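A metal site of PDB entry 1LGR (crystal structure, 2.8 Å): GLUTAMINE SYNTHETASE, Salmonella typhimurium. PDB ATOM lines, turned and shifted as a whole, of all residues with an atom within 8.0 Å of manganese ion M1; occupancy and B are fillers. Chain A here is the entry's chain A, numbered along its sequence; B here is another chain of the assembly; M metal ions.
N of Glu 212 is in hydrogen-bond range of O of Gln 218.
The backbone carbonyl oxygen of Glu 212 sits at hydrogen-bond distance from the backbone NH of Tyr 179 (3.2 Å).
N of Glu 220 lies within hydrogen-bond range of O of His 210, 2.8 Å away.
The side-chain carboxylate (OE1) of Glu 131 is in hydrogen-bond range of the backbone NH (N) of Gly 267, at 2.8 Å.
Of the 22 residues printed, 3 come within 4 Å of manganese ion M1.
The nearest printed residue that does not touch manganese ion M1 is His 210 (4.7 Å).
Manganese ion M1 is bound by OE2 of Glu 131, OE1 of Glu 220 and OE2 of Glu 212.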
ATOM      1  N   GLU A 129      24.528  -6.428 -22.406  1.00  0.00           N
ATOM      2  CA  GLU A 129      23.580  -7.458 -22.854  1.00  0.00           C
ATOM      3  C   GLU A 129      22.248  -6.767 -23.245  1.00  0.00           C
ATOM      4  O   GLU A 129      21.290  -6.873 -22.445  1.00  0.00           O
ATOM      5  CB  GLU A 129      23.357  -8.502 -21.701  1.00  0.00           C
ATOM      6  CG  GLU A 129      24.484  -9.289 -20.986  1.00  0.00           C
ATOM      7  CD  GLU A 129      24.068 -10.053 -19.685  1.00  0.00           C
ATOM      8  OE1 GLU A 129      23.609  -9.448 -18.702  1.00  0.00           O
ATOM      9  OE2 GLU A 129      24.182 -11.287 -19.629  1.00  0.00           O
ATOM     10  N   PRO A 130      22.103  -6.024 -24.360  1.00  0.00           N
ATOM     11  CA  PRO A 130      20.914  -5.281 -24.759  1.00  0.00           C
ATOM     12  C   PRO A 130      19.744  -6.165 -25.134  1.00  0.00           C
ATOM     13  O   PRO A 130      19.898  -7.148 -25.875  1.00  0.00           O
ATOM     14  CB  PRO A 130      21.299  -4.409 -25.931  1.00  0.00           C
ATOM     15  CG  PRO A 130      22.779  -4.547 -26.007  1.00  0.00           C
ATOM     16  CD  PRO A 130      23.015  -5.968 -25.486  1.00  0.00           C
ATOM     17  N   GLU A 131      18.562  -5.923 -24.568  1.00  0.00           N
ATOM     18  CA  GLU A 131      17.390  -6.669 -25.008  1.00  0.00           C
ATOM     19  C   GLU A 131      16.477  -5.801 -25.836  1.00  0.00           C
ATOM     20  O   GLU A 131      16.427  -4.585 -25.690  1.00  0.00           O
ATOM     21  CB  GLU A 131      16.615  -7.158 -23.849  1.00  0.00           C
ATOM     22  CG  GLU A 131      17.483  -8.132 -23.110  1.00  0.00           C
ATOM     23  CD  GLU A 131      17.056  -8.371 -21.674  1.00  0.00           C
ATOM     24  OE1 GLU A 131      16.609  -7.441 -20.989  1.00  0.00           O
ATOM     25  OE2 GLU A 131      17.163  -9.490 -21.220  1.00  0.00           O
ATOM     26  N   PHE A 132      15.700  -6.423 -26.710  1.00  0.00           N
ATOM     27  CA  PHE A 132      14.774  -5.648 -27.522  1.00  0.00           C
ATOM     28  C   PHE A 132      13.402  -6.281 -27.663  1.00  0.00           C
ATOM     29  O   PHE A 132      13.185  -7.438 -27.291  1.00  0.00           O
ATOM     30  CB  PHE A 132      15.372  -5.401 -28.913  1.00  0.00           C
ATOM     31  CG  PHE A 132      15.782  -6.606 -29.728  1.00  0.00           C
ATOM     32  CD1 PHE A 132      17.062  -7.163 -29.577  1.00  0.00           C
ATOM     33  CD2 PHE A 132      14.892  -7.172 -30.641  1.00  0.00           C
ATOM     34  CE1 PHE A 132      17.437  -8.268 -30.337  1.00  0.00           C
ATOM     35  CE2 PHE A 132      15.274  -8.266 -31.399  1.00  0.00           C
ATOM     36  CZ  PHE A 132      16.540  -8.822 -31.252  1.00  0.00           C
ATOM     37  N   TYR A 179      10.470 -17.196 -22.364  1.00  0.00           N
ATOM     38  CA  TYR A 179      11.733 -17.832 -22.097  1.00  0.00           C
ATOM     39  C   TYR A 179      11.812 -19.346 -22.236  1.00  0.00           C
ATOM     40  O   TYR A 179      11.480 -20.217 -21.433  1.00  0.00           O
ATOM     41  CB  TYR A 179      12.188 -17.411 -20.737  1.00  0.00           C
ATOM     42  CG  TYR A 179      13.706 -17.434 -20.672  1.00  0.00           C
ATOM     43  CD1 TYR A 179      14.462 -16.313 -21.041  1.00  0.00           C
ATOM     44  CD2 TYR A 179      14.320 -18.589 -20.205  1.00  0.00           C
ATOM     45  CE1 TYR A 179      15.854 -16.353 -20.944  1.00  0.00           C
ATOM     46  CE2 TYR A 179      15.704 -18.649 -20.105  1.00  0.00           C
ATOM     47  CZ  TYR A 179      16.460 -17.529 -20.475  1.00  0.00           C
ATOM     48  OH  TYR A 179      17.840 -17.608 -20.389  1.00  0.00           O
ATOM     49  N   HIS A 210      18.649 -15.703 -28.371  1.00  0.00           N
ATOM     50  CA  HIS A 210      17.487 -16.409 -27.874  1.00  0.00           C
ATOM     51  C   HIS A 210      16.325 -15.465 -27.610  1.00  0.00           C
ATOM     52  O   HIS A 210      16.502 -14.256 -27.465  1.00  0.00           O
ATOM     53  CB  HIS A 210      17.790 -17.129 -26.578  1.00  0.00           C
ATOM     54  CG  HIS A 210      18.232 -16.184 -25.491  1.00  0.00           C
ATOM     55  ND1 HIS A 210      17.469 -15.568 -24.599  1.00  0.00           N
ATOM     56  CD2 HIS A 210      19.521 -15.778 -25.298  1.00  0.00           C
ATOM     57  CE1 HIS A 210      18.248 -14.824 -23.892  1.00  0.00           C
ATOM     58  NE2 HIS A 210      19.480 -14.943 -24.302  1.00  0.00           N
ATOM     59  N   HIS A 211      15.146 -16.039 -27.483  1.00  0.00           N
ATOM     60  CA  HIS A 211      13.968 -15.291 -27.059  1.00  0.00           C
ATOM     61  C   HIS A 211      14.065 -14.964 -25.571  1.00  0.00           C
ATOM     62  O   HIS A 211      14.628 -15.711 -24.765  1.00  0.00           O
ATOM     63  CB  HIS A 211      12.723 -16.124 -27.314  1.00  0.00           C
ATOM     64  CG  HIS A 211      11.421 -15.349 -27.251  1.00  0.00           C
ATOM     65  ND1 HIS A 211      10.922 -14.545 -26.322  1.00  0.00           N
ATOM     66  CD2 HIS A 211      10.491 -15.404 -28.252  1.00  0.00           C
ATOM     67  CE1 HIS A 211       9.751 -14.113 -26.701  1.00  0.00           C
ATOM     68  NE2 HIS A 211       9.518 -14.652 -27.858  1.00  0.00           N
ATOM     69  N   GLU A 212      13.605 -13.795 -25.178  1.00  0.00           N
ATOM     70  CA  GLU A 212      13.580 -13.438 -23.775  1.00  0.00           C
ATOM     71  C   GLU A 212      12.276 -13.747 -23.040  1.00  0.00           C
ATOM     72  O   GLU A 212      11.385 -14.346 -23.620  1.00  0.00           O
ATOM     73  CB  GLU A 212      13.923 -11.971 -23.663  1.00  0.00           C
ATOM     74  CG  GLU A 212      15.322 -11.803 -23.130  1.00  0.00           C
ATOM     75  CD  GLU A 212      15.583 -12.348 -21.718  1.00  0.00           C
ATOM     76  OE1 GLU A 212      14.673 -12.532 -20.915  1.00  0.00           O
ATOM     77  OE2 GLU A 212      16.750 -12.585 -21.391  1.00  0.00           O
ATOM     78  N   VAL A 213      12.086 -13.303 -21.814  1.00  0.00           N
ATOM     79  CA  VAL A 213      10.953 -13.703 -20.984  1.00  0.00           C
ATOM     80  C   VAL A 213       9.568 -13.263 -21.413  1.00  0.00           C
ATOM     81  O   VAL A 213       8.585 -13.982 -21.288  1.00  0.00           O
ATOM     82  CB  VAL A 213      11.274 -13.228 -19.556  1.00  0.00           C
ATOM     83  CG1 VAL A 213      10.081 -13.166 -18.631  1.00  0.00           C
ATOM     84  CG2 VAL A 213      12.209 -14.245 -18.962  1.00  0.00           C
ATOM     85  N   GLN A 218       9.892 -10.352 -26.977  1.00  0.00           N
ATOM     86  CA  GLN A 218      11.168  -9.948 -26.406  1.00  0.00           C
ATOM     87  C   GLN A 218      12.290 -10.869 -26.876  1.00  0.00           C
ATOM     88  O   GLN A 218      12.172 -12.101 -26.828  1.00  0.00           O
ATOM     89  CB  GLN A 218      11.132  -9.984 -24.910  1.00  0.00           C
ATOM     90  CG  GLN A 218      12.046  -8.852 -24.460  1.00  0.00           C
ATOM     91  CD  GLN A 218      12.189  -8.764 -22.942  1.00  0.00           C
ATOM     92  OE1 GLN A 218      11.972  -9.742 -22.220  1.00  0.00           O
ATOM     93  NE2 GLN A 218      12.572  -7.629 -22.393  1.00  0.00           N
ATOM     94  N   ASN A 219      13.380 -10.298 -27.362  1.00  0.00           N
ATOM     95  CA  ASN A 219      14.503 -11.069 -27.879  1.00  0.00           C
ATOM     96  C   ASN A 219      15.879 -10.585 -27.457  1.00  0.00           C
ATOM     97  O   ASN A 219      16.044  -9.461 -26.972  1.00  0.00           O
ATOM     98  CB  ASN A 219      14.453 -11.073 -29.387  1.00  0.00           C
ATOM     99  CG  ASN A 219      13.349 -11.986 -29.847  1.00  0.00           C
ATOM    100  OD1 ASN A 219      12.238 -11.628 -30.153  1.00  0.00           O
ATOM    101  ND2 ASN A 219      13.534 -13.276 -29.841  1.00  0.00           N
ATOM    102  N   GLU A 220      16.887 -11.440 -27.601  1.00  0.00           N
ATOM    103  CA  GLU A 220      18.238 -11.055 -27.232  1.00  0.00           C
ATOM    104  C   GLU A 220      19.284 -11.693 -28.116  1.00  0.00           C
ATOM    105  O   GLU A 220      19.293 -12.905 -28.326  1.00  0.00           O
ATOM    106  CB  GLU A 220      18.518 -11.453 -25.826  1.00  0.00           C
ATOM    107  CG  GLU A 220      19.722 -10.820 -25.155  1.00  0.00           C
ATOM    108  CD  GLU A 220      19.817 -11.216 -23.684  1.00  0.00           C
ATOM    109  OE1 GLU A 220      18.797 -11.528 -23.084  1.00  0.00           O
ATOM    110  OE2 GLU A 220      20.920 -11.214 -23.124  1.00  0.00           O
ATOM    111  N   VAL A 221      20.163 -10.869 -28.640  1.00  0.00           N
ATOM    112  CA  VAL A 221      21.327 -11.362 -29.348  1.00  0.00           C
ATOM    113  C   VAL A 221      22.531 -11.030 -28.452  1.00  0.00           C
ATOM    114  O   VAL A 221      22.828  -9.870 -28.158  1.00  0.00           O
ATOM    115  CB  VAL A 221      21.470 -10.682 -30.731  1.00  0.00           C
ATOM    116  CG1 VAL A 221      22.724 -11.181 -31.421  1.00  0.00           C
ATOM    117  CG2 VAL A 221      20.260 -11.004 -31.574  1.00  0.00           C
ATOM    118  N   ASN A 264       7.986  -8.460 -18.592  1.00  0.00           N
ATOM    119  CA  ASN A 264       9.355  -8.037 -18.677  1.00  0.00           C
ATOM    120  C   ASN A 264       9.728  -6.768 -19.439  1.00  0.00           C
ATOM    121  O   ASN A 264       9.154  -6.371 -20.451  1.00  0.00           O
ATOM    122  CB  ASN A 264      10.108  -9.233 -19.239  1.00  0.00           C
ATOM    123  CG  ASN A 264      11.461  -9.410 -18.586  1.00  0.00           C
ATOM    124  OD1 ASN A 264      12.502  -9.555 -19.190  1.00  0.00           O
ATOM    125  ND2 ASN A 264      11.501  -9.438 -17.267  1.00  0.00           N
ATOM    126  N   GLY A 265      10.719  -6.122 -18.848  1.00  0.00           N
ATOM    127  CA  GLY A 265      11.319  -4.964 -19.454  1.00  0.00           C
ATOM    128  C   GLY A 265      12.637  -5.367 -20.105  1.00  0.00           C
ATOM    129  O   GLY A 265      13.262  -6.401 -19.863  1.00  0.00           O
ATOM    130  N   SER A 266      13.009  -4.535 -21.038  1.00  0.00           N
ATOM    131  CA  SER A 266      14.270  -4.690 -21.728  1.00  0.00           C
ATOM    132  C   SER A 266      15.360  -3.926 -20.974  1.00  0.00           C
ATOM    133  O   SER A 266      15.335  -2.695 -20.815  1.00  0.00           O
ATOM    134  CB  SER A 266      14.119  -4.166 -23.142  1.00  0.00           C
ATOM    135  OG  SER A 266      13.301  -5.091 -23.826  1.00  0.00           O
ATOM    136  N   GLY A 267      16.268  -4.681 -20.369  1.00  0.00           N
ATOM    137  CA  GLY A 267      17.453  -4.090 -19.771  1.00  0.00           C
ATOM    138  C   GLY A 267      18.728  -4.330 -20.575  1.00  0.00           C
ATOM    139  O   GLY A 267      18.810  -5.224 -21.427  1.00  0.00           O
ATOM    140  N   MET A 268      19.769  -3.536 -20.329  1.00  0.00           N
ATOM    141  CA  MET A 268      21.068  -3.730 -20.975  1.00  0.00           C
ATOM    142  C   MET A 268      22.134  -3.901 -19.895  1.00  0.00           C
ATOM    143  O   MET A 268      22.753  -2.952 -19.423  1.00  0.00           O
ATOM    144  CB  MET A 268      21.446  -2.542 -21.847  1.00  0.00           C
ATOM    145  CG  MET A 268      22.729  -2.696 -22.646  1.00  0.00           C
ATOM    146  SD  MET A 268      23.359  -1.044 -22.999  1.00  0.00           S
ATOM    147  CE  MET A 268      22.781  -0.849 -24.649  1.00  0.00           C
ATOM    148  N   HIS A 269      22.379  -5.125 -19.475  1.00  0.00           N
ATOM    149  CA  HIS A 269      23.339  -5.296 -18.386  1.00  0.00           C
ATOM    150  C   HIS A 269      24.769  -5.136 -18.862  1.00  0.00           C
ATOM    151  O   HIS A 269      25.190  -5.799 -19.816  1.00  0.00           O
ATOM    152  CB  HIS A 269      23.332  -6.668 -17.742  1.00  0.00           C
ATOM    153  CG  HIS A 269      22.002  -7.210 -17.258  1.00  0.00           C
ATOM    154  ND1 HIS A 269      21.823  -8.129 -16.314  1.00  0.00           N
ATOM    155  CD2 HIS A 269      20.780  -6.795 -17.698  1.00  0.00           C
ATOM    156  CE1 HIS A 269      20.525  -8.252 -16.202  1.00  0.00           C
ATOM    157  NE2 HIS A 269      19.907  -7.464 -17.016  1.00  0.00           N
ATOM    158  N   ARG A 339      20.219 -12.468  -7.192  1.00  0.00           N
ATOM    159  CA  ARG A 339      19.740 -11.747  -8.403  1.00  0.00           C
ATOM    160  C   ARG A 339      18.478 -10.987  -7.965  1.00  0.00           C
ATOM    161  O   ARG A 339      17.320 -11.383  -8.044  1.00  0.00           O
ATOM    162  CB  ARG A 339      19.344 -12.684  -9.580  1.00  0.00           C
ATOM    163  CG  ARG A 339      20.378 -13.675 -10.112  1.00  0.00           C
ATOM    164  CD  ARG A 339      20.911 -13.474 -11.540  1.00  0.00           C
ATOM    165  NE  ARG A 339      19.972 -13.666 -12.652  1.00  0.00           N
ATOM    166  CZ  ARG A 339      20.356 -14.217 -13.820  1.00  0.00           C
ATOM    167  NH1 ARG A 339      21.550 -14.764 -14.009  1.00  0.00           N
ATOM    168  NH2 ARG A 339      19.487 -14.239 -14.828  1.00  0.00           N
ATOM    169  N   ARG A 359      23.580  -4.968 -13.358  1.00  0.00           N
ATOM    170  CA  ARG A 359      22.288  -5.285 -13.947  1.00  0.00           C
ATOM    171  C   ARG A 359      21.307  -4.157 -14.219  1.00  0.00           C
ATOM    172  O   ARG A 359      20.390  -4.378 -15.003  1.00  0.00           O
ATOM    173  CB  ARG A 359      21.547  -6.278 -13.096  1.00  0.00           C
ATOM    174  CG  ARG A 359      22.286  -7.563 -12.919  1.00  0.00           C
ATOM    175  CD  ARG A 359      21.330  -8.575 -12.394  1.00  0.00           C
ATOM    176  NE  ARG A 359      21.397  -9.788 -13.187  1.00  0.00           N
ATOM    177  CZ  ARG A 359      20.325 -10.310 -13.794  1.00  0.00           C
ATOM    178  NH1 ARG A 359      19.141  -9.682 -13.915  1.00  0.00           N
ATOM    179  NH2 ARG A 359      20.467 -11.458 -14.420  1.00  0.00           N
ATOM    180  N   ASP B  50      20.879 -18.983 -17.397  1.00  0.00           N
ATOM    181  CA  ASP B  50      20.058 -18.760 -16.235  1.00  0.00           C
ATOM    182  C   ASP B  50      18.844 -19.677 -16.192  1.00  0.00           C
ATOM    183  O   ASP B  50      17.779 -19.482 -16.769  1.00  0.00           O
ATOM    184  CB  ASP B  50      19.603 -17.321 -16.173  1.00  0.00           C
ATOM    185  CG  ASP B  50      18.887 -17.066 -14.850  1.00  0.00           C
ATOM    186  OD1 ASP B  50      19.481 -17.294 -13.789  1.00  0.00           O
ATOM    187  OD2 ASP B  50      17.734 -16.642 -14.908  1.00  0.00           O
HETATM  188 MN    MN M   1      18.452 -11.141 -20.993  1.00  0.00          MN
HETATM  189 MN    MN M   2      23.148 -10.936 -16.951  1.00  0.00          MN
